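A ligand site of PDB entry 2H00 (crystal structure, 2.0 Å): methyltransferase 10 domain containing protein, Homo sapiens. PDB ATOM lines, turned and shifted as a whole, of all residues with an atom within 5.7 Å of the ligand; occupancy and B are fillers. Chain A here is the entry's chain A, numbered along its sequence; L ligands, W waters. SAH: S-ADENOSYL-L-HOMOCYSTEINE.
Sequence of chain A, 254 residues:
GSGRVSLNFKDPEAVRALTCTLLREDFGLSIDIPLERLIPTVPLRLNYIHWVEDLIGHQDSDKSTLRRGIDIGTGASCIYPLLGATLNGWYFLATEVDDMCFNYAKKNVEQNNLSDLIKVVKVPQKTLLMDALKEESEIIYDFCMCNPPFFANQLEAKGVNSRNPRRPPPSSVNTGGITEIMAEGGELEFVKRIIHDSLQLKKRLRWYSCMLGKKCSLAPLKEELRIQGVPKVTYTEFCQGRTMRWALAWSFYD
The backbone carbonyl oxygen of Thr 127 sits at hydrogen-bond distance from a nitrogen (N6) of the ligand (2.8 Å). An oxygen (O3') of the ligand sits at hydrogen-bond distance from the side-chain sulfur of Cys 101. NE2 of Gln 125 sits close to N6 of the ligand, 3.4 Å away. OE1 of Glu 96 is in hydrogen-bond range of O3' of the ligand, 2.6 Å away. A nitrogen (N) of the ligand is in hydrogen-bond range of the backbone carbonyl oxygen (O) of Gly 73 (2.8 Å). NE of Arg 45 lies within salt-bridge range of O of the ligand. The side-chain amide nitrogen (ND2) of Asn 147 lies within hydrogen-bond range of an oxygen (O) of the ligand, at 3.0 Å. A nitrogen (N3) of the ligand sits close to the backbone NH (N) of Gly 73 (3.4 Å). O of Thr 74 is in hydrogen-bond range of N of the ligand, at 3.4 Å.
The backbone NH (N) of Thr 95 sits at hydrogen-bond distance from the backbone carbonyl oxygen (O) of Asp 71 (3.0 Å). The backbone NH (N) of Ile 79 lies within hydrogen-bond range of the side-chain hydroxyl (OG) of Ser 77, at 3.0 Å. The side-chain hydroxyl of Thr 127 sits at hydrogen-bond distance from the backbone carbonyl oxygen of Pro 124, at 2.6 Å. The backbone carbonyl oxygen of Gln 125 sits at hydrogen-bond distance from the guanidinium group of Arg 193. OD2 of Asp 71 sits at hydrogen-bond distance from OG1 of Thr 74 (2.9 Å). OE1 of Glu 96 sits at hydrogen-bond distance from N of Thr 74, at 3.5 Å. The side-chain carboxylate (OD2) of Asp 98 is in salt-bridge range of the guanidinium group (NE) of Arg 37, at 2.8 Å. The side-chain sulfur of Cys 101 lies within hydrogen-bond range of the backbone NH of Ala 76, 3.6 Å away.
Residues that only touch the ligand: Leu 38 (3.7 Å), Pro 40 (3.7 Å), Gly 75 (3.7 Å), Ile 79 (3.9 Å), Tyr 80 (3.7 Å), Thr 95 (3.5 Å), Val 97 (3.6 Å), Asp 98 (3.5 Å), Val 123 (3.8 Å), Leu 128 (3.4 Å), Pro 149 (3.4 Å), Phe 151 (3.7 Å), Phe 190 (3.6 Å) and Arg 193 (3.6 Å). Hydrophobic or aromatic side chains within 4 Å of the ligand: Leu 38, Pro 40, Ile 79, Tyr 80, Val 97, Val 123, Leu 128, Pro 149, Phe 151 and Phe 190. Within 4 Å of the ligand: Leu 38, Pro 40, Arg 45, Gly 73, Thr 74, Gly 75, Ile 79, Tyr 80, Thr 95, Glu 96, Val 97, Asp 98, Cys 101, Val 123, Gln 125, Thr 127, Leu 128, Asn 147, Pro 149, Phe 151, Phe 190 and Arg 193. The nearest printed residue that does not touch the ligand is Pro 148 (4.1 Å).
Water W4 lies within hydrogen-bond range of an oxygen (OXT) of the ligand, the side-chain hydroxyl (OG) of Ser 77 and the backbone carbonyl oxygen (O) of Leu 38. Water W1 lies within hydrogen-bond range of the side-chain carboxylate of Asp 71, the backbone carbonyl oxygen of Thr 74, a nitrogen (N) of the ligand, the backbone NH of Tyr 80 and the backbone NH of Ile 79. Water W2 lies within hydrogen-bond range of OG1 of Thr 95 (2.8 Å), N1 of the ligand (2.9 Å) and O of Leu 128 (3.0 Å).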
ATOM      1  N   ARG A  37     -12.878  37.312 -11.350  1.00  0.00           N
ATOM      2  CA  ARG A  37     -13.248  36.102 -10.540  1.00  0.00           C
ATOM      3  C   ARG A  37     -12.031  35.298 -10.192  1.00  0.00           C
ATOM      4  O   ARG A  37     -10.977  35.478 -10.789  1.00  0.00           O
ATOM      5  CB  ARG A  37     -14.292  35.206 -11.280  1.00  0.00           C
ATOM      6  CG  ARG A  37     -15.600  35.932 -11.730  1.00  0.00           C
ATOM      7  CD  ARG A  37     -16.516  35.971 -10.569  1.00  0.00           C
ATOM      8  NE  ARG A  37     -17.759  36.702 -10.739  1.00  0.00           N
ATOM      9  CZ  ARG A  37     -17.974  38.008 -10.585  1.00  0.00           C
ATOM     10  NH1 ARG A  37     -16.977  38.859 -10.258  1.00  0.00           N
ATOM     11  NH2 ARG A  37     -19.199  38.459 -10.756  1.00  0.00           N
ATOM     12  N   LEU A  38     -12.165  34.423  -9.184  1.00  0.00           N
ATOM     13  CA  LEU A  38     -11.135  33.604  -8.645  1.00  0.00           C
ATOM     14  C   LEU A  38     -10.448  32.900  -9.781  1.00  0.00           C
ATOM     15  O   LEU A  38     -11.130  32.246 -10.623  1.00  0.00           O
ATOM     16  CB  LEU A  38     -11.733  32.565  -7.657  1.00  0.00           C
ATOM     17  CG  LEU A  38     -10.830  31.442  -7.126  1.00  0.00           C
ATOM     18  CD1 LEU A  38      -9.626  31.952  -6.298  1.00  0.00           C
ATOM     19  CD2 LEU A  38     -11.652  30.447  -6.246  1.00  0.00           C
ATOM     20  N   ILE A  39      -9.117  33.046  -9.806  1.00  0.00           N
ATOM     21  CA  ILE A  39      -8.230  32.491 -10.825  1.00  0.00           C
ATOM     22  C   ILE A  39      -7.751  31.203 -10.143  1.00  0.00           C
ATOM     23  O   ILE A  39      -7.042  31.262  -9.157  1.00  0.00           O
ATOM     24  CB  ILE A  39      -6.954  33.402 -11.125  1.00  0.00           C
ATOM     25  CG1 ILE A  39      -7.357  34.821 -11.614  1.00  0.00           C
ATOM     26  CG2 ILE A  39      -5.950  32.713 -12.038  1.00  0.00           C
ATOM     27  CD1 ILE A  39      -8.237  34.869 -12.877  1.00  0.00           C
ATOM     28  N   PRO A  40      -8.198  30.031 -10.648  1.00  0.00           N
ATOM     29  CA  PRO A  40      -7.774  28.810  -9.975  1.00  0.00           C
ATOM     30  C   PRO A  40      -6.284  28.531 -10.152  1.00  0.00           C
ATOM     31  O   PRO A  40      -5.682  28.885 -11.158  1.00  0.00           O
ATOM     32  CB  PRO A  40      -8.631  27.707 -10.649  1.00  0.00           C
ATOM     33  CG  PRO A  40      -8.820  28.172 -12.007  1.00  0.00           C
ATOM     34  CD  PRO A  40      -9.061  29.731 -11.829  1.00  0.00           C
ATOM     35  N   ARG A  45      -6.077  22.089  -7.559  1.00  0.00           N
ATOM     36  CA  ARG A  45      -7.319  21.558  -8.185  1.00  0.00           C
ATOM     37  C   ARG A  45      -7.113  20.076  -8.575  1.00  0.00           C
ATOM     38  O   ARG A  45      -8.029  19.256  -8.412  1.00  0.00           O
ATOM     39  CB  ARG A  45      -7.776  22.370  -9.387  1.00  0.00           C
ATOM     40  CG  ARG A  45      -8.077  23.847  -9.149  1.00  0.00           C
ATOM     41  CD  ARG A  45      -8.907  24.070  -7.891  1.00  0.00           C
ATOM     42  NE  ARG A  45      -9.455  25.415  -7.829  1.00  0.00           N
ATOM     43  CZ  ARG A  45      -8.816  26.453  -7.223  1.00  0.00           C
ATOM     44  NH1 ARG A  45      -9.402  27.651  -7.141  1.00  0.00           N
ATOM     45  NH2 ARG A  45      -7.646  26.239  -6.651  1.00  0.00           N
ATOM     46  N   ASP A  71     -20.287  19.383  -9.288  1.00  0.00           N
ATOM     47  CA  ASP A  71     -19.331  20.405  -8.757  1.00  0.00           C
ATOM     48  C   ASP A  71     -20.173  21.599  -8.386  1.00  0.00           C
ATOM     49  O   ASP A  71     -20.695  22.232  -9.250  1.00  0.00           O
ATOM     50  CB  ASP A  71     -18.317  20.768  -9.811  1.00  0.00           C
ATOM     51  CG  ASP A  71     -17.337  21.903  -9.355  1.00  0.00           C
ATOM     52  OD1 ASP A  71     -17.155  22.082  -8.141  1.00  0.00           O
ATOM     53  OD2 ASP A  71     -16.725  22.507 -10.228  1.00  0.00           O
ATOM     54  N   ILE A  72     -20.350  21.836  -7.092  1.00  0.00           N
ATOM     55  CA  ILE A  72     -21.092  23.006  -6.563  1.00  0.00           C
ATOM     56  C   ILE A  72     -20.200  24.285  -6.645  1.00  0.00           C
ATOM     57  O   ILE A  72     -19.167  24.333  -5.972  1.00  0.00           O
ATOM     58  CB  ILE A  72     -21.438  22.782  -5.046  1.00  0.00           C
ATOM     59  CG1 ILE A  72     -22.196  21.423  -4.831  1.00  0.00           C
ATOM     60  CG2 ILE A  72     -22.209  24.008  -4.444  1.00  0.00           C
ATOM     61  CD1 ILE A  72     -21.979  20.863  -3.369  1.00  0.00           C
ATOM     62  N   GLY A  73     -20.590  25.252  -7.458  1.00  0.00           N
ATOM     63  CA  GLY A  73     -19.901  26.554  -7.494  1.00  0.00           C
ATOM     64  C   GLY A  73     -18.715  26.388  -8.406  1.00  0.00           C
ATOM     65  O   GLY A  73     -17.578  26.407  -7.957  1.00  0.00           O
ATOM     66  N   THR A  74     -19.021  26.162  -9.675  1.00  0.00           N
ATOM     67  CA  THR A  74     -18.038  25.711 -10.640  1.00  0.00           C
ATOM     68  C   THR A  74     -17.041  26.794 -11.118  1.00  0.00           C
ATOM     69  O   THR A  74     -15.945  26.437 -11.513  1.00  0.00           O
ATOM     70  CB  THR A  74     -18.682  25.004 -11.897  1.00  0.00           C
ATOM     71  OG1 THR A  74     -17.684  24.131 -12.437  1.00  0.00           O
ATOM     72  CG2 THR A  74     -19.077  26.048 -13.048  1.00  0.00           C
ATOM     73  N   GLY A  75     -17.404  28.083 -11.016  1.00  0.00           N
ATOM     74  CA  GLY A  75     -16.440  29.176 -11.286  1.00  0.00           C
ATOM     75  C   GLY A  75     -16.451  29.519 -12.757  1.00  0.00           C
ATOM     76  O   GLY A  75     -17.097  28.834 -13.584  1.00  0.00           O
ATOM     77  N   ALA A  76     -15.773  30.604 -13.118  1.00  0.00           N
ATOM     78  CA  ALA A  76     -15.662  31.004 -14.488  1.00  0.00           C
ATOM     79  C   ALA A  76     -14.838  29.987 -15.279  1.00  0.00           C
ATOM     80  O   ALA A  76     -15.095  29.806 -16.450  1.00  0.00           O
ATOM     81  CB  ALA A  76     -15.030  32.454 -14.644  1.00  0.00           C
ATOM     82  N   SER A  77     -13.854  29.400 -14.621  1.00  0.00           N
ATOM     83  CA  SER A  77     -12.904  28.439 -15.211  1.00  0.00           C
ATOM     84  C   SER A  77     -13.586  27.047 -15.539  1.00  0.00           C
ATOM     85  O   SER A  77     -13.088  26.314 -16.404  1.00  0.00           O
ATOM     86  CB  SER A  77     -11.744  28.258 -14.261  1.00  0.00           C
ATOM     87  OG  SER A  77     -12.081  27.483 -13.068  1.00  0.00           O
ATOM     88  N   ILE A  79     -13.184  24.699 -13.626  1.00  0.00           N
ATOM     89  CA  ILE A  79     -11.973  23.946 -13.545  1.00  0.00           C
ATOM     90  C   ILE A  79     -12.092  22.454 -13.144  1.00  0.00           C
ATOM     91  O   ILE A  79     -11.409  21.607 -13.743  1.00  0.00           O
ATOM     92  CB  ILE A  79     -10.851  24.605 -12.688  1.00  0.00           C
ATOM     93  CG1 ILE A  79      -9.560  23.761 -12.824  1.00  0.00           C
ATOM     94  CG2 ILE A  79     -11.234  24.667 -11.185  1.00  0.00           C
ATOM     95  CD1 ILE A  79      -8.804  23.849 -14.165  1.00  0.00           C
ATOM     96  N   TYR A  80     -12.859  22.155 -12.112  1.00  0.00           N
ATOM     97  CA  TYR A  80     -12.908  20.777 -11.703  1.00  0.00           C
ATOM     98  C   TYR A  80     -13.573  19.883 -12.796  1.00  0.00           C
ATOM     99  O   TYR A  80     -13.005  18.860 -13.110  1.00  0.00           O
ATOM    100  CB  TYR A  80     -13.526  20.515 -10.329  1.00  0.00           C
ATOM    101  CG  TYR A  80     -12.851  21.135  -9.103  1.00  0.00           C
ATOM    102  CD1 TYR A  80     -11.566  20.749  -8.701  1.00  0.00           C
ATOM    103  CD2 TYR A  80     -13.565  21.987  -8.250  1.00  0.00           C
ATOM    104  CE1 TYR A  80     -11.028  21.204  -7.527  1.00  0.00           C
ATOM    105  CE2 TYR A  80     -12.989  22.515  -7.070  1.00  0.00           C
ATOM    106  CZ  TYR A  80     -11.714  22.114  -6.748  1.00  0.00           C
ATOM    107  OH  TYR A  80     -11.160  22.593  -5.603  1.00  0.00           O
ATOM    108  N   THR A  95     -22.739  23.426 -11.063  1.00  0.00           N
ATOM    109  CA  THR A  95     -23.663  24.522 -10.785  1.00  0.00           C
ATOM    110  C   THR A  95     -22.947  25.847 -10.515  1.00  0.00           C
ATOM    111  O   THR A  95     -21.804  25.832 -10.053  1.00  0.00           O
ATOM    112  CB  THR A  95     -24.567  24.205  -9.583  1.00  0.00           C
ATOM    113  OG1 THR A  95     -23.765  24.012  -8.433  1.00  0.00           O
ATOM    114  CG2 THR A  95     -25.354  22.899  -9.800  1.00  0.00           C
ATOM    115  N   GLU A  96     -23.647  26.953 -10.799  1.00  0.00           N
ATOM    116  CA  GLU A  96     -23.198  28.341 -10.469  1.00  0.00           C
ATOM    117  C   GLU A  96     -24.426  29.147 -10.106  1.00  0.00           C
ATOM    118  O   GLU A  96     -25.513  28.865 -10.632  1.00  0.00           O
ATOM    119  CB  GLU A  96     -22.536  29.052 -11.657  1.00  0.00           C
ATOM    120  CG  GLU A  96     -21.037  29.311 -11.513  1.00  0.00           C
ATOM    121  CD  GLU A  96     -20.659  29.966 -10.196  1.00  0.00           C
ATOM    122  OE1 GLU A  96     -19.631  29.608  -9.659  1.00  0.00           O
ATOM    123  OE2 GLU A  96     -21.417  30.815  -9.667  1.00  0.00           O
ATOM    124  N   VAL A  97     -24.252  30.144  -9.227  1.00  0.00           N
ATOM    125  CA  VAL A  97     -25.261  31.182  -9.015  1.00  0.00           C
ATOM    126  C   VAL A  97     -24.858  32.487  -9.689  1.00  0.00           C
ATOM    127  O   VAL A  97     -25.716  33.304  -9.997  1.00  0.00           O
ATOM    128  CB  VAL A  97     -25.561  31.454  -7.510  1.00  0.00           C
ATOM    129  CG1 VAL A  97     -26.154  30.222  -6.876  1.00  0.00           C
ATOM    130  CG2 VAL A  97     -24.301  31.952  -6.725  1.00  0.00           C
ATOM    131  N   ASP A  98     -23.562  32.685  -9.931  1.00  0.00           N
ATOM    132  CA  ASP A  98     -23.056  33.943 -10.501  1.00  0.00           C
ATOM    133  C   ASP A  98     -23.198  34.006 -12.038  1.00  0.00           C
ATOM    134  O   ASP A  98     -22.706  33.128 -12.743  1.00  0.00           O
ATOM    135  CB  ASP A  98     -21.616  34.184 -10.055  1.00  0.00           C
ATOM    136  CG  ASP A  98     -21.055  35.519 -10.559  1.00  0.00           C
ATOM    137  OD1 ASP A  98     -21.531  36.576 -10.096  1.00  0.00           O
ATOM    138  OD2 ASP A  98     -20.174  35.507 -11.450  1.00  0.00           O
ATOM    139  N   CYS A 101     -19.768  34.034 -13.915  1.00  0.00           N
ATOM    140  CA  CYS A 101     -19.103  32.744 -13.862  1.00  0.00           C
ATOM    141  C   CYS A 101     -19.821  31.673 -14.785  1.00  0.00           C
ATOM    142  O   CYS A 101     -19.181  30.879 -15.482  1.00  0.00           O
ATOM    143  CB  CYS A 101     -19.033  32.221 -12.431  1.00  0.00           C
ATOM    144  SG  CYS A 101     -17.715  32.988 -11.343  1.00  0.00           S
ATOM    145  N   VAL A 123     -28.326  27.825 -10.968  1.00  0.00           N
ATOM    146  CA  VAL A 123     -29.320  27.530  -9.929  1.00  0.00           C
ATOM    147  C   VAL A 123     -29.723  28.845  -9.228  1.00  0.00           C
ATOM    148  O   VAL A 123     -29.086  29.872  -9.459  1.00  0.00           O
ATOM    149  CB  VAL A 123     -28.763  26.463  -8.921  1.00  0.00           C
ATOM    150  CG1 VAL A 123     -28.316  25.231  -9.687  1.00  0.00           C
ATOM    151  CG2 VAL A 123     -27.620  27.024  -8.048  1.00  0.00           C
ATOM    152  N   PRO A 124     -30.801  28.849  -8.428  1.00  0.00           N
ATOM    153  CA  PRO A 124     -31.066  30.054  -7.589  1.00  0.00           C
ATOM    154  C   PRO A 124     -30.253  30.050  -6.283  1.00  0.00           C
ATOM    155  O   PRO A 124     -29.917  28.979  -5.779  1.00  0.00           O
ATOM    156  CB  PRO A 124     -32.566  29.971  -7.342  1.00  0.00           C
ATOM    157  CG  PRO A 124     -32.894  28.503  -7.408  1.00  0.00           C
ATOM    158  CD  PRO A 124     -31.840  27.818  -8.289  1.00  0.00           C
ATOM    159  N   GLN A 125     -29.905  31.225  -5.735  1.00  0.00           N
ATOM    160  CA  GLN A 125     -28.851  31.335  -4.679  1.00  0.00           C
ATOM    161  C   GLN A 125     -29.222  30.729  -3.325  1.00  0.00           C
ATOM    162  O   GLN A 125     -28.345  30.342  -2.520  1.00  0.00           O
ATOM    163  CB  GLN A 125     -28.361  32.788  -4.499  1.00  0.00           C
ATOM    164  CG  GLN A 125     -26.803  32.957  -4.324  1.00  0.00           C
ATOM    165  CD  GLN A 125     -26.241  32.541  -2.945  1.00  0.00           C
ATOM    166  OE1 GLN A 125     -26.016  33.403  -2.074  1.00  0.00           O
ATOM    167  NE2 GLN A 125     -25.977  31.239  -2.752  1.00  0.00           N
ATOM    168  N   LYS A 126     -30.517  30.610  -3.058  1.00  0.00           N
ATOM    169  CA  LYS A 126     -30.918  29.875  -1.852  1.00  0.00           C
ATOM    170  C   LYS A 126     -30.843  28.358  -2.035  1.00  0.00           C
ATOM    171  O   LYS A 126     -31.211  27.609  -1.128  1.00  0.00           O
ATOM    172  CB  LYS A 126     -32.308  30.303  -1.366  1.00  0.00           C
ATOM    173  N   THR A 127     -30.328  27.902  -3.168  1.00  0.00           N
ATOM    174  CA  THR A 127     -30.295  26.452  -3.418  1.00  0.00           C
ATOM    175  C   THR A 127     -28.877  25.867  -3.424  1.00  0.00           C
ATOM    176  O   THR A 127     -27.887  26.585  -3.658  1.00  0.00           O
ATOM    177  CB  THR A 127     -31.091  26.011  -4.692  1.00  0.00           C
ATOM    178  OG1 THR A 127     -30.433  26.466  -5.870  1.00  0.00           O
ATOM    179  CG2 THR A 127     -32.543  26.525  -4.668  1.00  0.00           C
ATOM    180  N   LEU A 128     -28.811  24.571  -3.147  1.00  0.00           N
ATOM    181  CA  LEU A 128     -27.577  23.858  -3.150  1.00  0.00           C
ATOM    182  C   LEU A 128     -27.688  22.558  -3.949  1.00  0.00           C
ATOM    183  O   LEU A 128     -27.687  22.646  -5.201  1.00  0.00           O
ATOM    184  CB  LEU A 128     -27.084  23.613  -1.720  1.00  0.00           C
ATOM    185  CG  LEU A 128     -25.574  23.796  -1.492  1.00  0.00           C
ATOM    186  CD1 LEU A 128     -25.150  25.234  -1.773  1.00  0.00           C
ATOM    187  CD2 LEU A 128     -25.252  23.477  -0.054  1.00  0.00           C
ATOM    188  N   ASN A 147     -15.319  23.741  -4.003  1.00  0.00           N
ATOM    189  CA  ASN A 147     -14.448  24.783  -3.400  1.00  0.00           C
ATOM    190  C   ASN A 147     -15.376  25.954  -2.971  1.00  0.00           C
ATOM    191  O   ASN A 147     -15.824  26.684  -3.790  1.00  0.00           O
ATOM    192  CB  ASN A 147     -13.415  25.206  -4.409  1.00  0.00           C
ATOM    193  CG  ASN A 147     -12.422  26.252  -3.840  1.00  0.00           C
ATOM    194  OD1 ASN A 147     -12.309  26.440  -2.619  1.00  0.00           O
ATOM    195  ND2 ASN A 147     -11.686  26.898  -4.749  1.00  0.00           N
ATOM    196  N   PRO A 148     -15.715  26.046  -1.668  1.00  0.00           N
ATOM    197  CA  PRO A 148     -16.758  26.948  -1.192  1.00  0.00           C
ATOM    198  C   PRO A 148     -16.462  28.483  -1.384  1.00  0.00           C
ATOM    199  O   PRO A 148     -15.294  28.879  -1.433  1.00  0.00           O
ATOM    200  CB  PRO A 148     -16.858  26.611   0.303  1.00  0.00           C
ATOM    201  CG  PRO A 148     -15.592  25.970   0.636  1.00  0.00           C
ATOM    202  CD  PRO A 148     -15.056  25.327  -0.588  1.00  0.00           C
ATOM    203  N   PRO A 149     -17.527  29.285  -1.568  1.00  0.00           N
ATOM    204  CA  PRO A 149     -17.331  30.735  -1.549  1.00  0.00           C
ATOM    205  C   PRO A 149     -17.108  31.271  -0.133  1.00  0.00           C
ATOM    206  O   PRO A 149     -17.381  30.593   0.883  1.00  0.00           O
ATOM    207  CB  PRO A 149     -18.636  31.288  -2.124  1.00  0.00           C
ATOM    208  CG  PRO A 149     -19.678  30.222  -1.743  1.00  0.00           C
ATOM    209  CD  PRO A 149     -18.945  28.901  -1.738  1.00  0.00           C
ATOM    210  N   PHE A 151     -18.348  34.093   1.921  1.00  0.00           N
ATOM    211  CA  PHE A 151     -19.451  35.041   2.074  1.00  0.00           C
ATOM    212  C   PHE A 151     -19.391  35.523   3.533  1.00  0.00           C
ATOM    213  O   PHE A 151     -19.237  36.737   3.756  1.00  0.00           O
ATOM    214  CB  PHE A 151     -20.825  34.406   1.812  1.00  0.00           C
ATOM    215  CG  PHE A 151     -21.120  34.095   0.370  1.00  0.00           C
ATOM    216  CD1 PHE A 151     -21.815  32.913   0.020  1.00  0.00           C
ATOM    217  CD2 PHE A 151     -20.755  34.986  -0.670  1.00  0.00           C
ATOM    218  CE1 PHE A 151     -22.135  32.630  -1.343  1.00  0.00           C
ATOM    219  CE2 PHE A 151     -21.048  34.694  -2.026  1.00  0.00           C
ATOM    220  CZ  PHE A 151     -21.741  33.517  -2.360  1.00  0.00           C
ATOM    221  N   PHE A 190     -21.414  27.579   4.927  1.00  0.00           N
ATOM    222  CA  PHE A 190     -21.589  26.941   3.628  1.00  0.00           C
ATOM    223  C   PHE A 190     -21.521  25.394   3.716  1.00  0.00           C
ATOM    224  O   PHE A 190     -22.405  24.710   3.237  1.00  0.00           O
ATOM    225  CB  PHE A 190     -20.649  27.492   2.551  1.00  0.00           C
ATOM    226  CG  PHE A 190     -21.095  27.175   1.140  1.00  0.00           C
ATOM    227  CD1 PHE A 190     -21.952  28.060   0.436  1.00  0.00           C
ATOM    228  CD2 PHE A 190     -20.690  25.993   0.524  1.00  0.00           C
ATOM    229  CE1 PHE A 190     -22.352  27.767  -0.852  1.00  0.00           C
ATOM    230  CE2 PHE A 190     -21.089  25.683  -0.787  1.00  0.00           C
ATOM    231  CZ  PHE A 190     -21.899  26.552  -1.470  1.00  0.00           C
ATOM    232  N   ARG A 193     -24.541  23.751   5.210  1.00  0.00           N
ATOM    233  CA  ARG A 193     -25.608  23.636   4.193  1.00  0.00           C
ATOM    234  C   ARG A 193     -25.496  22.356   3.330  1.00  0.00           C
ATOM    235  O   ARG A 193     -26.521  21.728   2.969  1.00  0.00           O
ATOM    236  CB  ARG A 193     -25.614  24.847   3.233  1.00  0.00           C
ATOM    237  CG  ARG A 193     -26.234  26.173   3.726  1.00  0.00           C
ATOM    238  CD  ARG A 193     -25.926  27.354   2.771  1.00  0.00           C
ATOM    239  NE  ARG A 193     -26.737  27.417   1.541  1.00  0.00           N
ATOM    240  CZ  ARG A 193     -26.511  28.226   0.503  1.00  0.00           C
ATOM    241  NH1 ARG A 193     -25.467  29.073   0.507  1.00  0.00           N
ATOM    242  NH2 ARG A 193     -27.298  28.198  -0.558  1.00  0.00           N
HETATM  243  N   SAH L   1     -14.847  25.895  -8.381  1.00  0.00           N
HETATM  244  CA  SAH L   1     -14.102  27.131  -8.760  1.00  0.00           C
HETATM  245  CB  SAH L   1     -14.802  28.379  -8.108  1.00  0.00           C
HETATM  246  CG  SAH L   1     -14.841  28.347  -6.591  1.00  0.00           C
HETATM  247  SD  SAH L   1     -15.299  29.922  -5.799  1.00  0.00           S
HETATM  248  C   SAH L   1     -12.625  27.008  -8.364  1.00  0.00           C
HETATM  249  O   SAH L   1     -12.195  26.103  -7.589  1.00  0.00           O
HETATM  250  OXT SAH L   1     -11.820  27.827  -8.835  1.00  0.00           O
HETATM  251  C5' SAH L   1     -16.974  29.365  -5.349  1.00  0.00           C
HETATM  252  C4' SAH L   1     -18.076  29.573  -6.419  1.00  0.00           C
HETATM  253  O4' SAH L   1     -19.291  29.134  -5.850  1.00  0.00           O
HETATM  254  C3' SAH L   1     -18.395  31.026  -6.845  1.00  0.00           C
HETATM  255  O3' SAH L   1     -18.232  31.224  -8.254  1.00  0.00           O
HETATM  256  C2' SAH L   1     -19.827  31.308  -6.438  1.00  0.00           C
HETATM  257  O2' SAH L   1     -20.442  32.095  -7.442  1.00  0.00           O
HETATM  258  C1' SAH L   1     -20.364  29.879  -6.383  1.00  0.00           C
HETATM  259  N9  SAH L   1     -21.516  29.674  -5.499  1.00  0.00           N
HETATM  260  C8  SAH L   1     -21.822  30.326  -4.323  1.00  0.00           C
HETATM  261  N7  SAH L   1     -22.980  29.792  -3.814  1.00  0.00           N
HETATM  262  C5  SAH L   1     -23.422  28.827  -4.652  1.00  0.00           C
HETATM  263  C6  SAH L   1     -24.549  27.983  -4.609  1.00  0.00           C
HETATM  264  N6  SAH L   1     -25.454  28.028  -3.625  1.00  0.00           N
HETATM  265  N1  SAH L   1     -24.720  27.117  -5.643  1.00  0.00           N
HETATM  266  C2  SAH L   1     -23.827  27.045  -6.704  1.00  0.00           C
HETATM  267  N3  SAH L   1     -22.715  27.854  -6.726  1.00  0.00           N
HETATM  268  C4  SAH L   1     -22.516  28.735  -5.718  1.00  0.00           C
HETATM  269  O   HOH W   1     -14.719  24.188 -10.685  1.00  0.00           O
HETATM  270  O   HOH W   2     -25.480  24.397  -6.235  1.00  0.00           O
HETATM  271  O   HOH W   3     -21.444  34.202  -5.910  1.00  0.00           O
HETATM  272  O   HOH W   4     -12.476  29.337 -11.001  1.00  0.00           O
HETATM  273  O   HOH W   5     -16.381  24.158  -6.552  1.00  0.00           O
